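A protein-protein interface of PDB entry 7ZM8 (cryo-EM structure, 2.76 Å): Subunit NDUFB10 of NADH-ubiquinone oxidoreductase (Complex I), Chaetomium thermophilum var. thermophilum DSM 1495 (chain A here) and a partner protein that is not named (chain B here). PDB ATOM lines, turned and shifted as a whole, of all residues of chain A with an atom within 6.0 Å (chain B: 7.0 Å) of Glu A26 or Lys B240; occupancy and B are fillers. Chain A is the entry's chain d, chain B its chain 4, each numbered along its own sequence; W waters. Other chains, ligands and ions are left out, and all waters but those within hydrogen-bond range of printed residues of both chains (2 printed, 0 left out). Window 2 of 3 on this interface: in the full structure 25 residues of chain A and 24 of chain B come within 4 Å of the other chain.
Glu A26 touches just one residue of chain B: Lys B240. Of chain A, only Tyr A25, Glu A26, Asn A28 and Leu A31 come within 4 Å of Lys B240. Printed residues of chain A within 4 Å of Ser B242: Gln A95 (3.2 Å). Of the printed residues of chain B, Gln A94 touches Leu B239 (3.9 Å). Of the printed residues of chain A, Leu B239 touches Gln A94 (3.9 Å). Ile B306 touches none of the printed residues of chain A. Asp B236 touches none of the printed residues of chain A. The nearest printed residue of chain B that does not touch Glu A26 is Val B237 (8.1 Å). The nearest residue of chain A that does not touch Lys B240 is Gln A94 (4.4 Å). The nearest printed residue of chain B that does not touch Gln A95 is Pro B305 (4.1 Å).
OG of Ser B242 lies within hydrogen-bond range of OE1 of Gln A95. O of Tyr A25 lies close to NZ of Lys B240 (3.4 Å).
Water W2 bridges OE1 of Gln A95 (2.7 Å) and OG of Ser B242 (3.2 Å). Water W1 bridges O of Leu B239 and NE2 of Gln A94.
The backbone NH (N) of Glu A26 sits close to the side-chain carboxylate (OD2) of Asp A24, 3.3 Å away. The side-chain hydroxyl (OH) of Tyr A25 lies within hydrogen-bond range of the backbone carbonyl oxygen (O) of Gln A94, 2.4 Å away. The backbone carbonyl oxygen of Glu A26 lies close to the side-chain amide oxygen of Asn A28, 3.5 Å away. The side-chain amide nitrogen of Gln A35 lies within hydrogen-bond range of the side-chain amide oxygen of Gln A94, at 2.7 Å.
Along chain B the printed residues that touch a printed residue of chain A span positions 239 to 242. Printed residues of chain A that touch a printed residue of chain B: Tyr A25, Glu A26, Asn A28, Leu A31, Gln A94 and Gln A95. Hydrophobic or aromatic side chains of chain A within 4 Å of the printed part of chain B: Leu A31. Among the printed residues, 6 pairs touch across the chains. Among the printed residues, no Asp or Glu carboxylate lies within 4 Å of a Lys or Arg side-chain nitrogen of the other chain.
Glu A26 touches Lys B240. Asn A28 touches Lys B240 (ND2 to CE, 3.8 Å). Leu A31 touches Lys B240. Leu B239 touches Gln A94 (O to NE2, 3.9 Å).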
ATOM      1  N   ASP A  24     -15.102 -20.549  33.143  1.00  0.00           N
ATOM      2  CA  ASP A  24     -14.502 -19.415  33.832  1.00  0.00           C
ATOM      3  C   ASP A  24     -13.044 -19.292  33.419  1.00  0.00           C
ATOM      4  O   ASP A  24     -12.270 -20.242  33.572  1.00  0.00           O
ATOM      5  CB  ASP A  24     -14.615 -19.586  35.343  1.00  0.00           C
ATOM      6  CG  ASP A  24     -13.919 -18.477  36.104  1.00  0.00           C
ATOM      7  OD1 ASP A  24     -14.466 -17.358  36.160  1.00  0.00           O
ATOM      8  OD2 ASP A  24     -12.820 -18.724  36.643  1.00  0.00           O
ATOM      9  N   TYR A  25     -12.670 -18.129  32.886  1.00  0.00           N
ATOM     10  CA  TYR A  25     -11.319 -17.981  32.359  1.00  0.00           C
ATOM     11  C   TYR A  25     -10.296 -17.894  33.480  1.00  0.00           C
ATOM     12  O   TYR A  25      -9.196 -18.446  33.363  1.00  0.00           O
ATOM     13  CB  TYR A  25     -11.237 -16.759  31.448  1.00  0.00           C
ATOM     14  CG  TYR A  25     -11.749 -17.014  30.051  1.00  0.00           C
ATOM     15  CD1 TYR A  25     -12.665 -18.021  29.802  1.00  0.00           C
ATOM     16  CD2 TYR A  25     -11.325 -16.247  28.984  1.00  0.00           C
ATOM     17  CE1 TYR A  25     -13.142 -18.253  28.537  1.00  0.00           C
ATOM     18  CE2 TYR A  25     -11.798 -16.474  27.713  1.00  0.00           C
ATOM     19  CZ  TYR A  25     -12.706 -17.478  27.499  1.00  0.00           C
ATOM     20  OH  TYR A  25     -13.180 -17.718  26.237  1.00  0.00           O
ATOM     21  N   GLU A  26     -10.644 -17.234  34.581  1.00  0.00           N
ATOM     22  CA  GLU A  26      -9.742 -17.153  35.721  1.00  0.00           C
ATOM     23  C   GLU A  26      -9.491 -18.508  36.370  1.00  0.00           C
ATOM     24  O   GLU A  26      -8.548 -18.627  37.158  1.00  0.00           O
ATOM     25  CB  GLU A  26     -10.292 -16.165  36.746  1.00  0.00           C
ATOM     26  CG  GLU A  26     -10.324 -14.735  36.237  1.00  0.00           C
ATOM     27  CD  GLU A  26     -10.481 -13.723  37.349  1.00  0.00           C
ATOM     28  OE1 GLU A  26     -10.711 -14.139  38.505  1.00  0.00           O
ATOM     29  OE2 GLU A  26     -10.371 -12.510  37.070  1.00  0.00           O
ATOM     30  N   ASP A  27     -10.283 -19.534  36.037  1.00  0.00           N
ATOM     31  CA  ASP A  27      -9.906 -20.908  36.451  1.00  0.00           C
ATOM     32  C   ASP A  27      -9.010 -21.354  35.308  1.00  0.00           C
ATOM     33  O   ASP A  27      -9.546 -21.759  34.281  1.00  0.00           O
ATOM     34  CB  ASP A  27     -11.099 -21.858  36.561  1.00  0.00           C
ATOM     35  CG  ASP A  27     -10.743 -23.280  36.957  1.00  0.00           C
ATOM     36  OD1 ASP A  27      -9.558 -23.542  37.233  1.00  0.00           O
ATOM     37  OD2 ASP A  27     -11.658 -24.114  36.989  1.00  0.00           O
ATOM     38  N   ASN A  28      -7.704 -21.297  35.504  1.00  0.00           N
ATOM     39  CA  ASN A  28      -6.719 -21.629  34.452  1.00  0.00           C
ATOM     40  C   ASN A  28      -6.798 -23.108  34.105  1.00  0.00           C
ATOM     41  O   ASN A  28      -6.694 -23.433  32.928  1.00  0.00           O
ATOM     42  CB  ASN A  28      -5.331 -21.205  34.924  1.00  0.00           C
ATOM     43  CG  ASN A  28      -5.323 -19.848  35.590  1.00  0.00           C
ATOM     44  OD1 ASN A  28      -5.257 -19.755  36.811  1.00  0.00           O
ATOM     45  ND2 ASN A  28      -5.392 -18.791  34.797  1.00  0.00           N
ATOM     46  N   LYS A  29      -6.950 -23.966  35.108  1.00  0.00           N
ATOM     47  CA  LYS A  29      -7.087 -25.423  34.880  1.00  0.00           C
ATOM     48  C   LYS A  29      -8.245 -25.701  33.907  1.00  0.00           C
ATOM     49  O   LYS A  29      -7.983 -26.354  32.896  1.00  0.00           O
ATOM     50  CB  LYS A  29      -7.140 -26.164  36.214  1.00  0.00           C
ATOM     51  CG  LYS A  29      -7.790 -27.544  36.209  1.00  0.00           C
ATOM     52  CD  LYS A  29      -7.065 -28.578  35.372  1.00  0.00           C
ATOM     53  CE  LYS A  29      -7.348 -29.997  35.812  1.00  0.00           C
ATOM     54  NZ  LYS A  29      -8.802 -30.260  35.916  1.00  0.00           N
ATOM     55  N   LEU A  31      -9.600 -23.724  31.849  1.00  0.00           N
ATOM     56  CA  LEU A  31      -9.397 -22.996  30.567  1.00  0.00           C
ATOM     57  C   LEU A  31      -8.421 -23.721  29.635  1.00  0.00           C
ATOM     58  O   LEU A  31      -8.719 -23.780  28.442  1.00  0.00           O
ATOM     59  CB  LEU A  31      -8.905 -21.584  30.881  1.00  0.00           C
ATOM     60  CG  LEU A  31      -8.497 -20.763  29.659  1.00  0.00           C
ATOM     61  CD1 LEU A  31      -9.705 -20.103  29.021  1.00  0.00           C
ATOM     62  CD2 LEU A  31      -7.448 -19.730  30.022  1.00  0.00           C
ATOM     63  N   GLN A  35      -8.804 -25.417  25.875  1.00  0.00           N
ATOM     64  CA  GLN A  35      -7.868 -25.139  24.763  1.00  0.00           C
ATOM     65  C   GLN A  35      -7.433 -26.481  24.187  1.00  0.00           C
ATOM     66  O   GLN A  35      -7.543 -26.653  22.971  1.00  0.00           O
ATOM     67  CB  GLN A  35      -6.713 -24.281  25.264  1.00  0.00           C
ATOM     68  CG  GLN A  35      -7.097 -22.851  25.603  1.00  0.00           C
ATOM     69  CD  GLN A  35      -5.920 -22.167  26.247  1.00  0.00           C
ATOM     70  OE1 GLN A  35      -4.873 -22.770  26.446  1.00  0.00           O
ATOM     71  NE2 GLN A  35      -6.079 -20.898  26.576  1.00  0.00           N
ATOM     72  N   GLN A  94     -11.753 -18.763  21.556  1.00  0.00           N
ATOM     73  CA  GLN A  94     -11.649 -18.328  22.944  1.00  0.00           C
ATOM     74  C   GLN A  94     -12.075 -16.882  23.132  1.00  0.00           C
ATOM     75  O   GLN A  94     -12.552 -16.520  24.209  1.00  0.00           O
ATOM     76  CB  GLN A  94     -10.216 -18.504  23.434  1.00  0.00           C
ATOM     77  CG  GLN A  94     -10.041 -18.304  24.916  1.00  0.00           C
ATOM     78  CD  GLN A  94      -8.605 -18.408  25.347  1.00  0.00           C
ATOM     79  OE1 GLN A  94      -8.240 -19.313  26.085  1.00  0.00           O
ATOM     80  NE2 GLN A  94      -7.780 -17.481  24.891  1.00  0.00           N
ATOM     81  N   GLN A  95     -11.901 -16.043  22.115  1.00  0.00           N
ATOM     82  CA  GLN A  95     -12.033 -14.601  22.255  1.00  0.00           C
ATOM     83  C   GLN A  95     -13.347 -14.052  21.734  1.00  0.00           C
ATOM     84  O   GLN A  95     -13.563 -12.841  21.812  1.00  0.00           O
ATOM     85  CB  GLN A  95     -10.893 -13.908  21.525  1.00  0.00           C
ATOM     86  CG  GLN A  95      -9.560 -14.005  22.198  1.00  0.00           C
ATOM     87  CD  GLN A  95      -8.515 -13.272  21.424  1.00  0.00           C
ATOM     88  OE1 GLN A  95      -8.834 -12.470  20.554  1.00  0.00           O
ATOM     89  NE2 GLN A  95      -7.258 -13.532  21.731  1.00  0.00           N
ATOM     90  N   PHE B 235       3.132 -14.856  30.579  1.00  0.00           N
ATOM     91  CA  PHE B 235       2.431 -15.302  29.347  1.00  0.00           C
ATOM     92  C   PHE B 235       1.038 -15.857  29.645  1.00  0.00           C
ATOM     93  O   PHE B 235       0.103 -15.454  28.951  1.00  0.00           O
ATOM     94  CB  PHE B 235       3.241 -16.388  28.632  1.00  0.00           C
ATOM     95  CG  PHE B 235       4.537 -15.964  27.989  1.00  0.00           C
ATOM     96  CD1 PHE B 235       4.764 -14.649  27.622  1.00  0.00           C
ATOM     97  CD2 PHE B 235       5.523 -16.899  27.720  1.00  0.00           C
ATOM     98  CE1 PHE B 235       5.958 -14.278  27.023  1.00  0.00           C
ATOM     99  CE2 PHE B 235       6.714 -16.526  27.122  1.00  0.00           C
ATOM    100  CZ  PHE B 235       6.932 -15.215  26.776  1.00  0.00           C
ATOM    101  N   ASP B 236       0.885 -16.704  30.661  1.00  0.00           N
ATOM    102  CA  ASP B 236      -0.435 -17.347  30.895  1.00  0.00           C
ATOM    103  C   ASP B 236      -1.530 -16.285  31.044  1.00  0.00           C
ATOM    104  O   ASP B 236      -2.606 -16.488  30.474  1.00  0.00           O
ATOM    105  CB  ASP B 236      -0.383 -18.328  32.063  1.00  0.00           C
ATOM    106  CG  ASP B 236       0.377 -19.605  31.749  1.00  0.00           C
ATOM    107  OD1 ASP B 236       0.515 -19.920  30.551  1.00  0.00           O
ATOM    108  OD2 ASP B 236       0.823 -20.274  32.704  1.00  0.00           O
ATOM    109  N   VAL B 237      -1.255 -15.190  31.749  1.00  0.00           N
ATOM    110  CA  VAL B 237      -2.267 -14.132  32.013  1.00  0.00           C
ATOM    111  C   VAL B 237      -2.410 -13.236  30.780  1.00  0.00           C
ATOM    112  O   VAL B 237      -3.532 -12.825  30.501  1.00  0.00           O
ATOM    113  CB  VAL B 237      -1.891 -13.353  33.289  1.00  0.00           C
ATOM    114  CG1 VAL B 237      -2.962 -12.358  33.693  1.00  0.00           C
ATOM    115  CG2 VAL B 237      -1.560 -14.288  34.438  1.00  0.00           C
ATOM    116  N   LEU B 238      -1.316 -12.973  30.057  1.00  0.00           N
ATOM    117  CA  LEU B 238      -1.403 -12.091  28.898  1.00  0.00           C
ATOM    118  C   LEU B 238      -2.123 -12.765  27.737  1.00  0.00           C
ATOM    119  O   LEU B 238      -2.853 -12.110  26.988  1.00  0.00           O
ATOM    120  CB  LEU B 238       0.002 -11.647  28.488  1.00  0.00           C
ATOM    121  CG  LEU B 238       0.225 -10.622  27.374  1.00  0.00           C
ATOM    122  CD1 LEU B 238      -0.558  -9.337  27.592  1.00  0.00           C
ATOM    123  CD2 LEU B 238       1.706 -10.327  27.252  1.00  0.00           C
ATOM    124  N   LEU B 239      -1.936 -14.075  27.572  1.00  0.00           N
ATOM    125  CA  LEU B 239      -2.550 -14.765  26.443  1.00  0.00           C
ATOM    126  C   LEU B 239      -4.055 -14.934  26.620  1.00  0.00           C
ATOM    127  O   LEU B 239      -4.780 -15.083  25.631  1.00  0.00           O
ATOM    128  CB  LEU B 239      -1.886 -16.124  26.227  1.00  0.00           C
ATOM    129  CG  LEU B 239      -0.372 -16.185  26.014  1.00  0.00           C
ATOM    130  CD1 LEU B 239       0.024 -17.549  25.475  1.00  0.00           C
ATOM    131  CD2 LEU B 239       0.145 -15.080  25.117  1.00  0.00           C
ATOM    132  N   LYS B 240      -4.546 -14.925  27.859  1.00  0.00           N
ATOM    133  CA  LYS B 240      -5.988 -14.944  28.074  1.00  0.00           C
ATOM    134  C   LYS B 240      -6.629 -13.640  27.619  1.00  0.00           C
ATOM    135  O   LYS B 240      -7.778 -13.626  27.166  1.00  0.00           O
ATOM    136  CB  LYS B 240      -6.300 -15.173  29.547  1.00  0.00           C
ATOM    137  CG  LYS B 240      -5.848 -16.485  30.095  1.00  0.00           C
ATOM    138  CD  LYS B 240      -5.742 -16.382  31.593  1.00  0.00           C
ATOM    139  CE  LYS B 240      -7.106 -16.517  32.208  1.00  0.00           C
ATOM    140  NZ  LYS B 240      -7.253 -15.703  33.436  1.00  0.00           N
ATOM    141  N   SER B 241      -5.908 -12.548  27.810  1.00  0.00           N
ATOM    142  CA  SER B 241      -6.462 -11.200  27.585  1.00  0.00           C
ATOM    143  C   SER B 241      -6.646 -10.843  26.111  1.00  0.00           C
ATOM    144  O   SER B 241      -5.743 -11.129  25.316  1.00  0.00           O
ATOM    145  CB  SER B 241      -5.539 -10.263  28.282  1.00  0.00           C
ATOM    146  OG  SER B 241      -5.521 -10.544  29.673  1.00  0.00           O
ATOM    147  N   SER B 242      -7.767 -10.225  25.766  1.00  0.00           N
ATOM    148  CA  SER B 242      -7.991  -9.773  24.377  1.00  0.00           C
ATOM    149  C   SER B 242      -8.043  -8.246  24.320  1.00  0.00           C
ATOM    150  O   SER B 242      -8.928  -7.655  24.945  1.00  0.00           O
ATOM    151  CB  SER B 242      -9.218 -10.395  23.796  1.00  0.00           C
ATOM    152  OG  SER B 242      -9.437  -9.932  22.475  1.00  0.00           O
ATOM    153  N   PRO B 305      -0.358 -14.496  19.347  1.00  0.00           N
ATOM    154  CA  PRO B 305      -1.383 -14.839  20.334  1.00  0.00           C
ATOM    155  C   PRO B 305      -2.143 -13.678  20.984  1.00  0.00           C
ATOM    156  O   PRO B 305      -3.214 -13.905  21.473  1.00  0.00           O
ATOM    157  CB  PRO B 305      -0.534 -15.584  21.370  1.00  0.00           C
ATOM    158  CG  PRO B 305       0.804 -14.892  21.348  1.00  0.00           C
ATOM    159  CD  PRO B 305       0.976 -14.379  19.936  1.00  0.00           C
ATOM    160  N   ILE B 306      -1.587 -12.472  20.954  1.00  0.00           N
ATOM    161  CA  ILE B 306      -2.156 -11.341  21.676  1.00  0.00           C
ATOM    162  C   ILE B 306      -2.551 -10.174  20.783  1.00  0.00           C
ATOM    163  O   ILE B 306      -3.293  -9.292  21.244  1.00  0.00           O
ATOM    164  CB  ILE B 306      -1.200 -10.861  22.788  1.00  0.00           C
ATOM    165  CG1 ILE B 306       0.117 -10.385  22.198  1.00  0.00           C
ATOM    166  CG2 ILE B 306      -0.960 -11.954  23.797  1.00  0.00           C
ATOM    167  CD1 ILE B 306       0.991  -9.705  23.189  1.00  0.00           C
HETATM  168  O   HOH W   1      -4.547 -17.910  25.290  1.00  0.00           O
HETATM  169  O   HOH W   2      -8.184  -9.998  19.580  1.00  0.00           O
